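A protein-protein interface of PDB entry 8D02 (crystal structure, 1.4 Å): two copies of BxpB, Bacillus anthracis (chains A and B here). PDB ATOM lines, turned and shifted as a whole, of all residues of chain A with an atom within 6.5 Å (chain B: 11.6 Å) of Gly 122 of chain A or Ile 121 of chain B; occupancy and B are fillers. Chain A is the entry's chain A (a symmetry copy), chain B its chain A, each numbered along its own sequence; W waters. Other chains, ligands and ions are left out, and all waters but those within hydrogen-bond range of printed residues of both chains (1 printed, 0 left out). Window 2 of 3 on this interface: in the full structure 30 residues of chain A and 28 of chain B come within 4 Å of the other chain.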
ATOM      1  N   LEU A  86       6.475 -13.782  18.774  1.00  0.00           N
ATOM      2  CA  LEU A  86       7.298 -12.566  18.862  1.00  0.00           C
ATOM      3  C   LEU A  86       8.127 -12.525  17.593  1.00  0.00           C
ATOM      4  O   LEU A  86       9.287 -12.981  17.606  1.00  0.00           O
ATOM      5  CB  LEU A  86       8.150 -12.647  20.104  1.00  0.00           C
ATOM      6  CG  LEU A  86       7.445 -12.847  21.447  1.00  0.00           C
ATOM      7  CD1 LEU A  86       8.476 -13.207  22.568  1.00  0.00           C
ATOM      8  CD2 LEU A  86       6.603 -11.634  21.841  1.00  0.00           C
ATOM      9  N   ASP A  87       7.552 -11.982  16.505  1.00  0.00           N
ATOM     10  CA  ASP A  87       8.203 -12.113  15.213  1.00  0.00           C
ATOM     11  C   ASP A  87       9.249 -11.035  14.960  1.00  0.00           C
ATOM     12  O   ASP A  87       9.897 -11.071  13.913  1.00  0.00           O
ATOM     13  CB  ASP A  87       7.174 -12.156  14.102  1.00  0.00           C
ATOM     14  CG  ASP A  87       6.335 -10.879  13.995  1.00  0.00           C
ATOM     15  OD1 ASP A  87       6.614  -9.898  14.717  1.00  0.00           O
ATOM     16  OD2 ASP A  87       5.382 -10.858  13.178  1.00  0.00           O
ATOM     17  N   ASN A  88       9.456 -10.091  15.873  1.00  0.00           N
ATOM     18  CA  ASN A  88      10.440  -9.033  15.727  1.00  0.00           C
ATOM     19  C   ASN A  88      10.056  -8.043  14.636  1.00  0.00           C
ATOM     20  O   ASN A  88      10.938  -7.331  14.128  1.00  0.00           O
ATOM     21  CB  ASN A  88      11.886  -9.553  15.596  1.00  0.00           C
ATOM     22  CG  ASN A  88      12.456  -9.987  16.911  1.00  0.00           C
ATOM     23  OD1 ASN A  88      11.942  -9.606  17.961  1.00  0.00           O
ATOM     24  ND2 ASN A  88      13.554 -10.730  16.867  1.00  0.00           N
ATOM     25  N   ALA A  92      12.464  -5.003  17.128  1.00  0.00           N
ATOM     26  CA  ALA A  92      13.117  -6.105  17.790  1.00  0.00           C
ATOM     27  C   ALA A  92      13.877  -5.574  18.993  1.00  0.00           C
ATOM     28  O   ALA A  92      14.524  -4.523  18.895  1.00  0.00           O
ATOM     29  CB  ALA A  92      14.084  -6.794  16.829  1.00  0.00           C
ATOM     30  N   ASN A 119      14.874 -12.723  21.075  1.00  0.00           N
ATOM     31  CA  ASN A 119      16.226 -12.273  20.781  1.00  0.00           C
ATOM     32  C   ASN A 119      16.160 -10.984  19.983  1.00  0.00           C
ATOM     33  O   ASN A 119      15.225 -10.755  19.213  1.00  0.00           O
ATOM     34  CB  ASN A 119      16.894 -13.318  19.914  1.00  0.00           C
ATOM     35  CG  ASN A 119      18.381 -13.286  20.027  1.00  0.00           C
ATOM     36  OD1 ASN A 119      19.011 -12.275  19.714  1.00  0.00           O
ATOM     37  ND2 ASN A 119      18.970 -14.377  20.510  1.00  0.00           N
ATOM     38  N   VAL A 120      17.167 -10.129  20.166  1.00  0.00           N
ATOM     39  CA  VAL A 120      17.189  -8.901  19.377  1.00  0.00           C
ATOM     40  C   VAL A 120      17.529  -9.188  17.913  1.00  0.00           C
ATOM     41  O   VAL A 120      17.154  -8.413  17.029  1.00  0.00           O
ATOM     42  CB  VAL A 120      18.109  -7.849  20.026  1.00  0.00           C
ATOM     43  CG1 VAL A 120      19.544  -8.352  20.036  1.00  0.00           C
ATOM     44  CG2 VAL A 120      17.970  -6.522  19.305  1.00  0.00           C
ATOM     45  N   ILE A 121      18.194 -10.309  17.624  1.00  0.00           N
ATOM     46  CA  ILE A 121      18.554 -10.702  16.265  1.00  0.00           C
ATOM     47  C   ILE A 121      17.499 -11.646  15.710  1.00  0.00           C
ATOM     48  O   ILE A 121      16.868 -12.407  16.447  1.00  0.00           O
ATOM     49  CB  ILE A 121      19.938 -11.379  16.282  1.00  0.00           C
ATOM     50  CG1 ILE A 121      20.949 -10.472  16.976  1.00  0.00           C
ATOM     51  CG2 ILE A 121      20.396 -11.721  14.879  1.00  0.00           C
ATOM     52  CD1 ILE A 121      20.982  -9.081  16.368  1.00  0.00           C
ATOM     53  N   GLY A 122      17.284 -11.603  14.415  1.00  0.00           N
ATOM     54  CA  GLY A 122      16.469 -12.592  13.724  1.00  0.00           C
ATOM     55  C   GLY A 122      14.960 -12.395  13.864  1.00  0.00           C
ATOM     56  O   GLY A 122      14.445 -11.287  14.159  1.00  0.00           O
ATOM     57  N   THR A 123      14.223 -13.469  13.573  1.00  0.00           N
ATOM     58  CA  THR A 123      12.766 -13.388  13.483  1.00  0.00           C
ATOM     59  C   THR A 123      12.182 -14.775  13.726  1.00  0.00           C
ATOM     60  O   THR A 123      12.872 -15.789  13.653  1.00  0.00           O
ATOM     61  CB  THR A 123      12.261 -12.894  12.097  1.00  0.00           C
ATOM     62  OG1 THR A 123      12.658 -13.807  11.054  1.00  0.00           O
ATOM     63  CG2 THR A 123      12.726 -11.434  11.735  1.00  0.00           C
ATOM     64  N   GLY A 124      10.873 -14.797  13.982  1.00  0.00           N
ATOM     65  CA  GLY A 124      10.124 -16.038  13.960  1.00  0.00           C
ATOM     66  C   GLY A 124       9.919 -16.764  15.282  1.00  0.00           C
ATOM     67  O   GLY A 124       9.285 -17.831  15.283  1.00  0.00           O
ATOM     68  N   GLU A 125      10.419 -16.251  16.401  1.00  0.00           N
ATOM     69  CA  GLU A 125      10.247 -16.995  17.650  1.00  0.00           C
ATOM     70  C   GLU A 125       8.785 -17.103  18.084  1.00  0.00           C
ATOM     71  O   GLU A 125       8.027 -16.129  18.034  1.00  0.00           O
ATOM     72  CB  GLU A 125      11.052 -16.351  18.758  1.00  0.00           C
ATOM     73  CG  GLU A 125      12.589 -16.445  18.591  1.00  0.00           C
ATOM     74  CD  GLU A 125      13.337 -15.536  19.549  1.00  0.00           C
ATOM     75  OE1 GLU A 125      14.001 -14.599  19.078  1.00  0.00           O
ATOM     76  OE2 GLU A 125      13.293 -15.815  20.776  1.00  0.00           O
ATOM     77  N   LEU B  86      15.097 -27.287  19.674  1.00  0.00           N
ATOM     78  CA  LEU B  86      14.961 -26.832  18.282  1.00  0.00           C
ATOM     79  C   LEU B  86      16.333 -26.339  17.863  1.00  0.00           C
ATOM     80  O   LEU B  86      16.595 -25.122  17.945  1.00  0.00           O
ATOM     81  CB  LEU B  86      13.917 -25.746  18.227  1.00  0.00           C
ATOM     82  CG  LEU B  86      12.521 -26.064  18.767  1.00  0.00           C
ATOM     83  CD1 LEU B  86      11.669 -24.758  18.910  1.00  0.00           C
ATOM     84  CD2 LEU B  86      11.797 -27.104  17.913  1.00  0.00           C
ATOM     85  N   ASP B  87      17.202 -27.261  17.412  1.00  0.00           N
ATOM     86  CA  ASP B  87      18.592 -26.891  17.207  1.00  0.00           C
ATOM     87  C   ASP B  87      18.848 -26.263  15.843  1.00  0.00           C
ATOM     88  O   ASP B  87      19.984 -25.870  15.574  1.00  0.00           O
ATOM     89  CB  ASP B  87      19.499 -28.081  17.446  1.00  0.00           C
ATOM     90  CG  ASP B  87      19.251 -29.243  16.480  1.00  0.00           C
ATOM     91  OD1 ASP B  87      18.442 -29.098  15.539  1.00  0.00           O
ATOM     92  OD2 ASP B  87      19.876 -30.317  16.665  1.00  0.00           O
ATOM     93  N   ASN B  88      17.845 -26.135  14.979  1.00  0.00           N
ATOM     94  CA  ASN B  88      17.990 -25.537  13.664  1.00  0.00           C
ATOM     95  C   ASN B  88      18.824 -26.404  12.731  1.00  0.00           C
ATOM     96  O   ASN B  88      19.357 -25.883  11.737  1.00  0.00           O
ATOM     97  CB  ASN B  88      18.453 -24.066  13.705  1.00  0.00           C
ATOM     98  CG  ASN B  88      17.344 -23.131  14.078  1.00  0.00           C
ATOM     99  OD1 ASN B  88      16.173 -23.493  13.979  1.00  0.00           O
ATOM    100  ND2 ASN B  88      17.698 -21.906  14.445  1.00  0.00           N
ATOM    101  N   SER B  89      18.918 -27.706  13.003  1.00  0.00           N
ATOM    102  CA  SER B  89      19.487 -28.639  12.039  1.00  0.00           C
ATOM    103  C   SER B  89      18.461 -29.752  11.849  1.00  0.00           C
ATOM    104  O   SER B  89      17.932 -30.304  12.842  1.00  0.00           O
ATOM    105  CB  SER B  89      20.770 -29.194  12.607  1.00  0.00           C
ATOM    106  OG  SER B  89      21.259 -30.209  11.716  1.00  0.00           O
ATOM    107  N   VAL B  91      17.160 -27.924   9.219  1.00  0.00           N
ATOM    108  CA  VAL B  91      16.507 -26.752   8.645  1.00  0.00           C
ATOM    109  C   VAL B  91      16.380 -25.729   9.762  1.00  0.00           C
ATOM    110  O   VAL B  91      16.354 -26.065  10.947  1.00  0.00           O
ATOM    111  CB  VAL B  91      15.087 -27.057   8.089  1.00  0.00           C
ATOM    112  CG1 VAL B  91      15.121 -28.118   6.945  1.00  0.00           C
ATOM    113  CG2 VAL B  91      14.095 -27.448   9.213  1.00  0.00           C
ATOM    114  N   ALA B  92      16.337 -24.455   9.374  1.00  0.00           N
ATOM    115  CA  ALA B  92      15.984 -23.397  10.288  1.00  0.00           C
ATOM    116  C   ALA B  92      14.863 -22.573   9.677  1.00  0.00           C
ATOM    117  O   ALA B  92      14.903 -22.279   8.475  1.00  0.00           O
ATOM    118  CB  ALA B  92      17.197 -22.506  10.550  1.00  0.00           C
ATOM    119  N   PRO B  93      13.843 -22.173  10.466  1.00  0.00           N
ATOM    120  CA  PRO B  93      13.639 -22.548  11.871  1.00  0.00           C
ATOM    121  C   PRO B  93      13.046 -23.941  11.975  1.00  0.00           C
ATOM    122  O   PRO B  93      12.758 -24.583  10.973  1.00  0.00           O
ATOM    123  CB  PRO B  93      12.615 -21.513  12.363  1.00  0.00           C
ATOM    124  CG  PRO B  93      11.867 -21.123  11.129  1.00  0.00           C
ATOM    125  CD  PRO B  93      12.853 -21.187   9.999  1.00  0.00           C
ATOM    126  N   GLU B  94      12.903 -24.412  13.209  1.00  0.00           N
ATOM    127  CA  GLU B  94      12.180 -25.635  13.527  1.00  0.00           C
ATOM    128  C   GLU B  94      10.972 -25.263  14.390  1.00  0.00           C
ATOM    129  O   GLU B  94      10.976 -24.224  15.060  1.00  0.00           O
ATOM    130  CB  GLU B  94      13.054 -26.671  14.195  1.00  0.00           C
ATOM    131  CG  GLU B  94      14.207 -27.076  13.246  1.00  0.00           C
ATOM    132  CD  GLU B  94      15.067 -28.173  13.785  1.00  0.00           C
ATOM    133  OE1 GLU B  94      15.653 -28.022  14.887  1.00  0.00           O
ATOM    134  OE2 GLU B  94      15.185 -29.216  13.109  1.00  0.00           O
ATOM    135  N   ARG B 117       8.462 -22.229  18.114  1.00  0.00           N
ATOM    136  CA  ARG B 117       9.239 -22.081  16.879  1.00  0.00           C
ATOM    137  C   ARG B 117      10.532 -21.370  17.233  1.00  0.00           C
ATOM    138  O   ARG B 117      10.528 -20.427  18.027  1.00  0.00           O
ATOM    139  CB  ARG B 117       8.431 -21.334  15.815  1.00  0.00           C
ATOM    140  CG  ARG B 117       9.228 -21.086  14.526  1.00  0.00           C
ATOM    141  CD  ARG B 117       8.333 -20.677  13.374  1.00  0.00           C
ATOM    142  NE  ARG B 117       7.892 -19.301  13.548  1.00  0.00           N
ATOM    143  CZ  ARG B 117       6.845 -18.741  12.960  1.00  0.00           C
ATOM    144  NH1 ARG B 117       6.185 -19.362  11.991  1.00  0.00           N
ATOM    145  NH2 ARG B 117       6.484 -17.496  13.309  1.00  0.00           N
ATOM    146  N   SER B 118      11.656 -21.837  16.672  1.00  0.00           N
ATOM    147  CA  SER B 118      12.958 -21.223  16.898  1.00  0.00           C
ATOM    148  C   SER B 118      13.128 -19.984  16.023  1.00  0.00           C
ATOM    149  O   SER B 118      12.379 -19.752  15.075  1.00  0.00           O
ATOM    150  CB  SER B 118      14.071 -22.250  16.630  1.00  0.00           C
ATOM    151  OG  SER B 118      13.988 -22.744  15.319  1.00  0.00           O
ATOM    152  N   ASN B 119      14.161 -19.218  16.362  1.00  0.00           N
ATOM    153  CA  ASN B 119      14.610 -18.138  15.495  1.00  0.00           C
ATOM    154  C   ASN B 119      15.168 -18.727  14.213  1.00  0.00           C
ATOM    155  O   ASN B 119      15.715 -19.831  14.201  1.00  0.00           O
ATOM    156  CB  ASN B 119      15.736 -17.409  16.195  1.00  0.00           C
ATOM    157  CG  ASN B 119      15.881 -16.000  15.725  1.00  0.00           C
ATOM    158  OD1 ASN B 119      16.133 -15.757  14.545  1.00  0.00           O
ATOM    159  ND2 ASN B 119      15.689 -15.043  16.630  1.00  0.00           N
ATOM    160  N   VAL B 120      15.029 -17.981  13.116  1.00  0.00           N
ATOM    161  CA  VAL B 120      15.602 -18.469  11.865  1.00  0.00           C
ATOM    162  C   VAL B 120      17.130 -18.384  11.885  1.00  0.00           C
ATOM    163  O   VAL B 120      17.799 -19.139  11.175  1.00  0.00           O
ATOM    164  CB  VAL B 120      14.963 -17.759  10.656  1.00  0.00           C
ATOM    165  CG1 VAL B 120      15.285 -16.274  10.699  1.00  0.00           C
ATOM    166  CG2 VAL B 120      15.427 -18.410   9.367  1.00  0.00           C
ATOM    167  N   ILE B 121      17.706 -17.513  12.716  1.00  0.00           N
ATOM    168  CA  ILE B 121      19.152 -17.358  12.842  1.00  0.00           C
ATOM    169  C   ILE B 121      19.658 -18.205  13.999  1.00  0.00           C
ATOM    170  O   ILE B 121      18.954 -18.428  14.987  1.00  0.00           O
ATOM    171  CB  ILE B 121      19.485 -15.871  13.066  1.00  0.00           C
ATOM    172  CG1 ILE B 121      18.843 -15.026  11.971  1.00  0.00           C
ATOM    173  CG2 ILE B 121      20.984 -15.647  13.109  1.00  0.00           C
ATOM    174  CD1 ILE B 121      19.217 -15.509  10.581  1.00  0.00           C
ATOM    175  N   GLY B 122      20.872 -18.695  13.892  1.00  0.00           N
ATOM    176  CA  GLY B 122      21.559 -19.333  15.006  1.00  0.00           C
ATOM    177  C   GLY B 122      21.129 -20.771  15.290  1.00  0.00           C
ATOM    178  O   GLY B 122      20.574 -21.497  14.427  1.00  0.00           O
ATOM    179  N   THR B 123      21.454 -21.227  16.502  1.00  0.00           N
ATOM    180  CA  THR B 123      21.274 -22.634  16.857  1.00  0.00           C
ATOM    181  C   THR B 123      21.158 -22.745  18.373  1.00  0.00           C
ATOM    182  O   THR B 123      21.512 -21.834  19.118  1.00  0.00           O
ATOM    183  CB  THR B 123      22.453 -23.540  16.401  1.00  0.00           C
ATOM    184  OG1 THR B 123      23.683 -23.139  17.039  1.00  0.00           O
ATOM    185  CG2 THR B 123      22.652 -23.586  14.840  1.00  0.00           C
ATOM    186  N   GLY B 124      20.684 -23.911  18.816  1.00  0.00           N
ATOM    187  CA  GLY B 124      20.773 -24.275  20.217  1.00  0.00           C
ATOM    188  C   GLY B 124      19.570 -23.982  21.102  1.00  0.00           C
ATOM    189  O   GLY B 124      19.629 -24.281  22.304  1.00  0.00           O
ATOM    190  N   GLU B 125      18.488 -23.417  20.578  1.00  0.00           N
ATOM    191  CA  GLU B 125      17.364 -23.104  21.462  1.00  0.00           C
ATOM    192  C   GLU B 125      16.704 -24.351  22.051  1.00  0.00           C
ATOM    193  O   GLU B 125      16.464 -25.342  21.353  1.00  0.00           O
ATOM    194  CB  GLU B 125      16.325 -22.291  20.721  1.00  0.00           C
ATOM    195  CG  GLU B 125      16.771 -20.861  20.328  1.00  0.00           C
ATOM    196  CD  GLU B 125      15.825 -20.207  19.337  1.00  0.00           C
ATOM    197  OE1 GLU B 125      16.248 -19.944  18.200  1.00  0.00           O
ATOM    198  OE2 GLU B 125      14.669 -19.908  19.740  1.00  0.00           O
ATOM    199  N   VAL B 126      16.411 -24.273  23.342  1.00  0.00           N
ATOM    200  CA  VAL B 126      15.626 -25.280  24.065  1.00  0.00           C
ATOM    201  C   VAL B 126      14.565 -24.536  24.850  1.00  0.00           C
ATOM    202  O   VAL B 126      14.865 -23.556  25.553  1.00  0.00           O
ATOM    203  CB  VAL B 126      16.479 -26.155  25.005  1.00  0.00           C
ATOM    204  CG1 VAL B 126      15.604 -27.228  25.709  1.00  0.00           C
ATOM    205  CG2 VAL B 126      17.598 -26.823  24.269  1.00  0.00           C
ATOM    206  N   ASP B 127      13.310 -24.972  24.691  1.00  0.00           N
ATOM    207  CA  ASP B 127      12.123 -24.307  25.215  1.00  0.00           C
ATOM    208  C   ASP B 127      11.276 -25.304  25.978  1.00  0.00           C
ATOM    209  O   ASP B 127      11.363 -26.498  25.746  1.00  0.00           O
ATOM    210  CB  ASP B 127      11.201 -23.792  24.086  1.00  0.00           C
ATOM    211  CG  ASP B 127      11.875 -22.804  23.112  1.00  0.00           C
ATOM    212  OD1 ASP B 127      12.827 -22.087  23.504  1.00  0.00           O
ATOM    213  OD2 ASP B 127      11.421 -22.740  21.925  1.00  0.00           O
HETATM  214  O   HOH W   1       7.014 -15.413  15.349  1.00  0.00           O
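NE of Arg 117 of chain B is in hydrogen-bond range of O of Gly 124 of chain A. The side-chain amide nitrogen (ND2) of Asn 119 of chain B sits at hydrogen-bond distance from the backbone carbonyl oxygen (O) of Ile 121 of chain A, 2.9 Å away. The side-chain amide oxygen (OD1) of Asn 119 of chain B lies within hydrogen-bond range of the backbone NH (N) of Thr 123 of chain A, 3.1 Å away. The side-chain amide nitrogen of Asn 119 of chain B sits at hydrogen-bond distance from the side-chain carboxylate of Glu 125 of chain A (3.0 Å). O of Thr 123 of chain A lies within hydrogen-bond range of N of Val 120 of chain B (3.1 Å).
N of Glu 94 of chain B sits at hydrogen-bond distance from OG of Ser 118 of chain B, 2.9 Å away. The backbone NH of Asn 119 of chain B is in hydrogen-bond range of the side-chain carboxylate of Glu 125 of chain B. The backbone NH (N) of Leu 86 of chain A sits at hydrogen-bond distance from the backbone carbonyl oxygen (O) of Glu 125 of chain A (2.9 Å). The backbone carbonyl oxygen (O) of Asn 119 of chain A is in hydrogen-bond range of the side-chain amide nitrogen (ND2) of Asn 88 of chain A (2.9 Å). The backbone carbonyl oxygen of Gly 122 of chain A sits at hydrogen-bond distance from the side-chain amide nitrogen of Asn 88 of chain A. The side-chain carboxylate (OE1) of Glu 125 of chain A sits at hydrogen-bond distance from the backbone NH (N) of Asn 119 of chain A (2.9 Å).
Among the printed residues, merely in contact across the chains: Asn 119 of chain A with Asn 119 of chain B (3.9 Å), Gly 122 of chain A with Asn 119 of chain B (3.3 Å), Gly 122 of chain A with Ile 121 of chain B (3.8 Å), Gly 124 of chain A with Ser 118 of chain B (3.6 Å) and Glu 125 of chain A with Arg 117 of chain B (3.5 Å).
Gly 122 of chain A touches just these residues of chain B: Asn 119 (3.3 Å) and Ile 121 (3.8 Å). Of chain A, only Gly 122 comes within 4 Å of Ile 121 of chain B. Printed residues of chain B within 4 Å of Asn 119 of chain A: Asn 119 (3.9 Å). Printed residues of chain A within 4 Å of Val 120 of chain B: Thr 123. Printed residues of chain A within 4 Å of Arg 117 of chain B: Gly 124 (2.7 Å) and Glu 125 (3.5 Å). Printed residues of chain A within 4 Å of Ser 118 of chain B: Gly 124 (3.6 Å). Printed residues of chain B within 4 Å of Gly 124 of chain A: Arg 117 (2.7 Å) and Ser 118 (3.6 Å). The nearest printed residue of chain B that does not touch Gly 122 of chain A is Val 120 of chain B (4.9 Å). The nearest printed residue of chain A that does not touch Arg 117 of chain B is Asp 87 of chain A (5.4 Å).
Of the 19 printed residues of chain B, 5 touch a printed residue of chain A. Among the printed residues, 10 pairs touch across the chains.
Ile 121 of chain A touches Asn 119 of chain B, but with the chains exchanged Asn 119 of chain A does not touch Ile 121 of chain B (6.8 Å). Gly 122 of chain A touches Asn 119 of chain B, but with the chains exchanged Asn 119 of chain A does not touch Gly 122 of chain B (7.8 Å). Gly 122 of chain A touches Ile 121 of chain B, but with the chains exchanged Ile 121 of chain A does not touch Gly 122 of chain B (7.1 Å). Thr 123 of chain A touches Val 120 of chain B, but with the chains exchanged Val 120 of chain A does not touch Thr 123 of chain B (12.4 Å). 11 positions are printed for both chains. Of the 10 pairs that touch across the chains among the printed residues, 1 has its exchanged pair printed and touching as well.
Water W1 lies within hydrogen-bond range of O of Glu 125 of chain A, NH2 of Arg 117 of chain B and O of Gly 124 of chain A.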
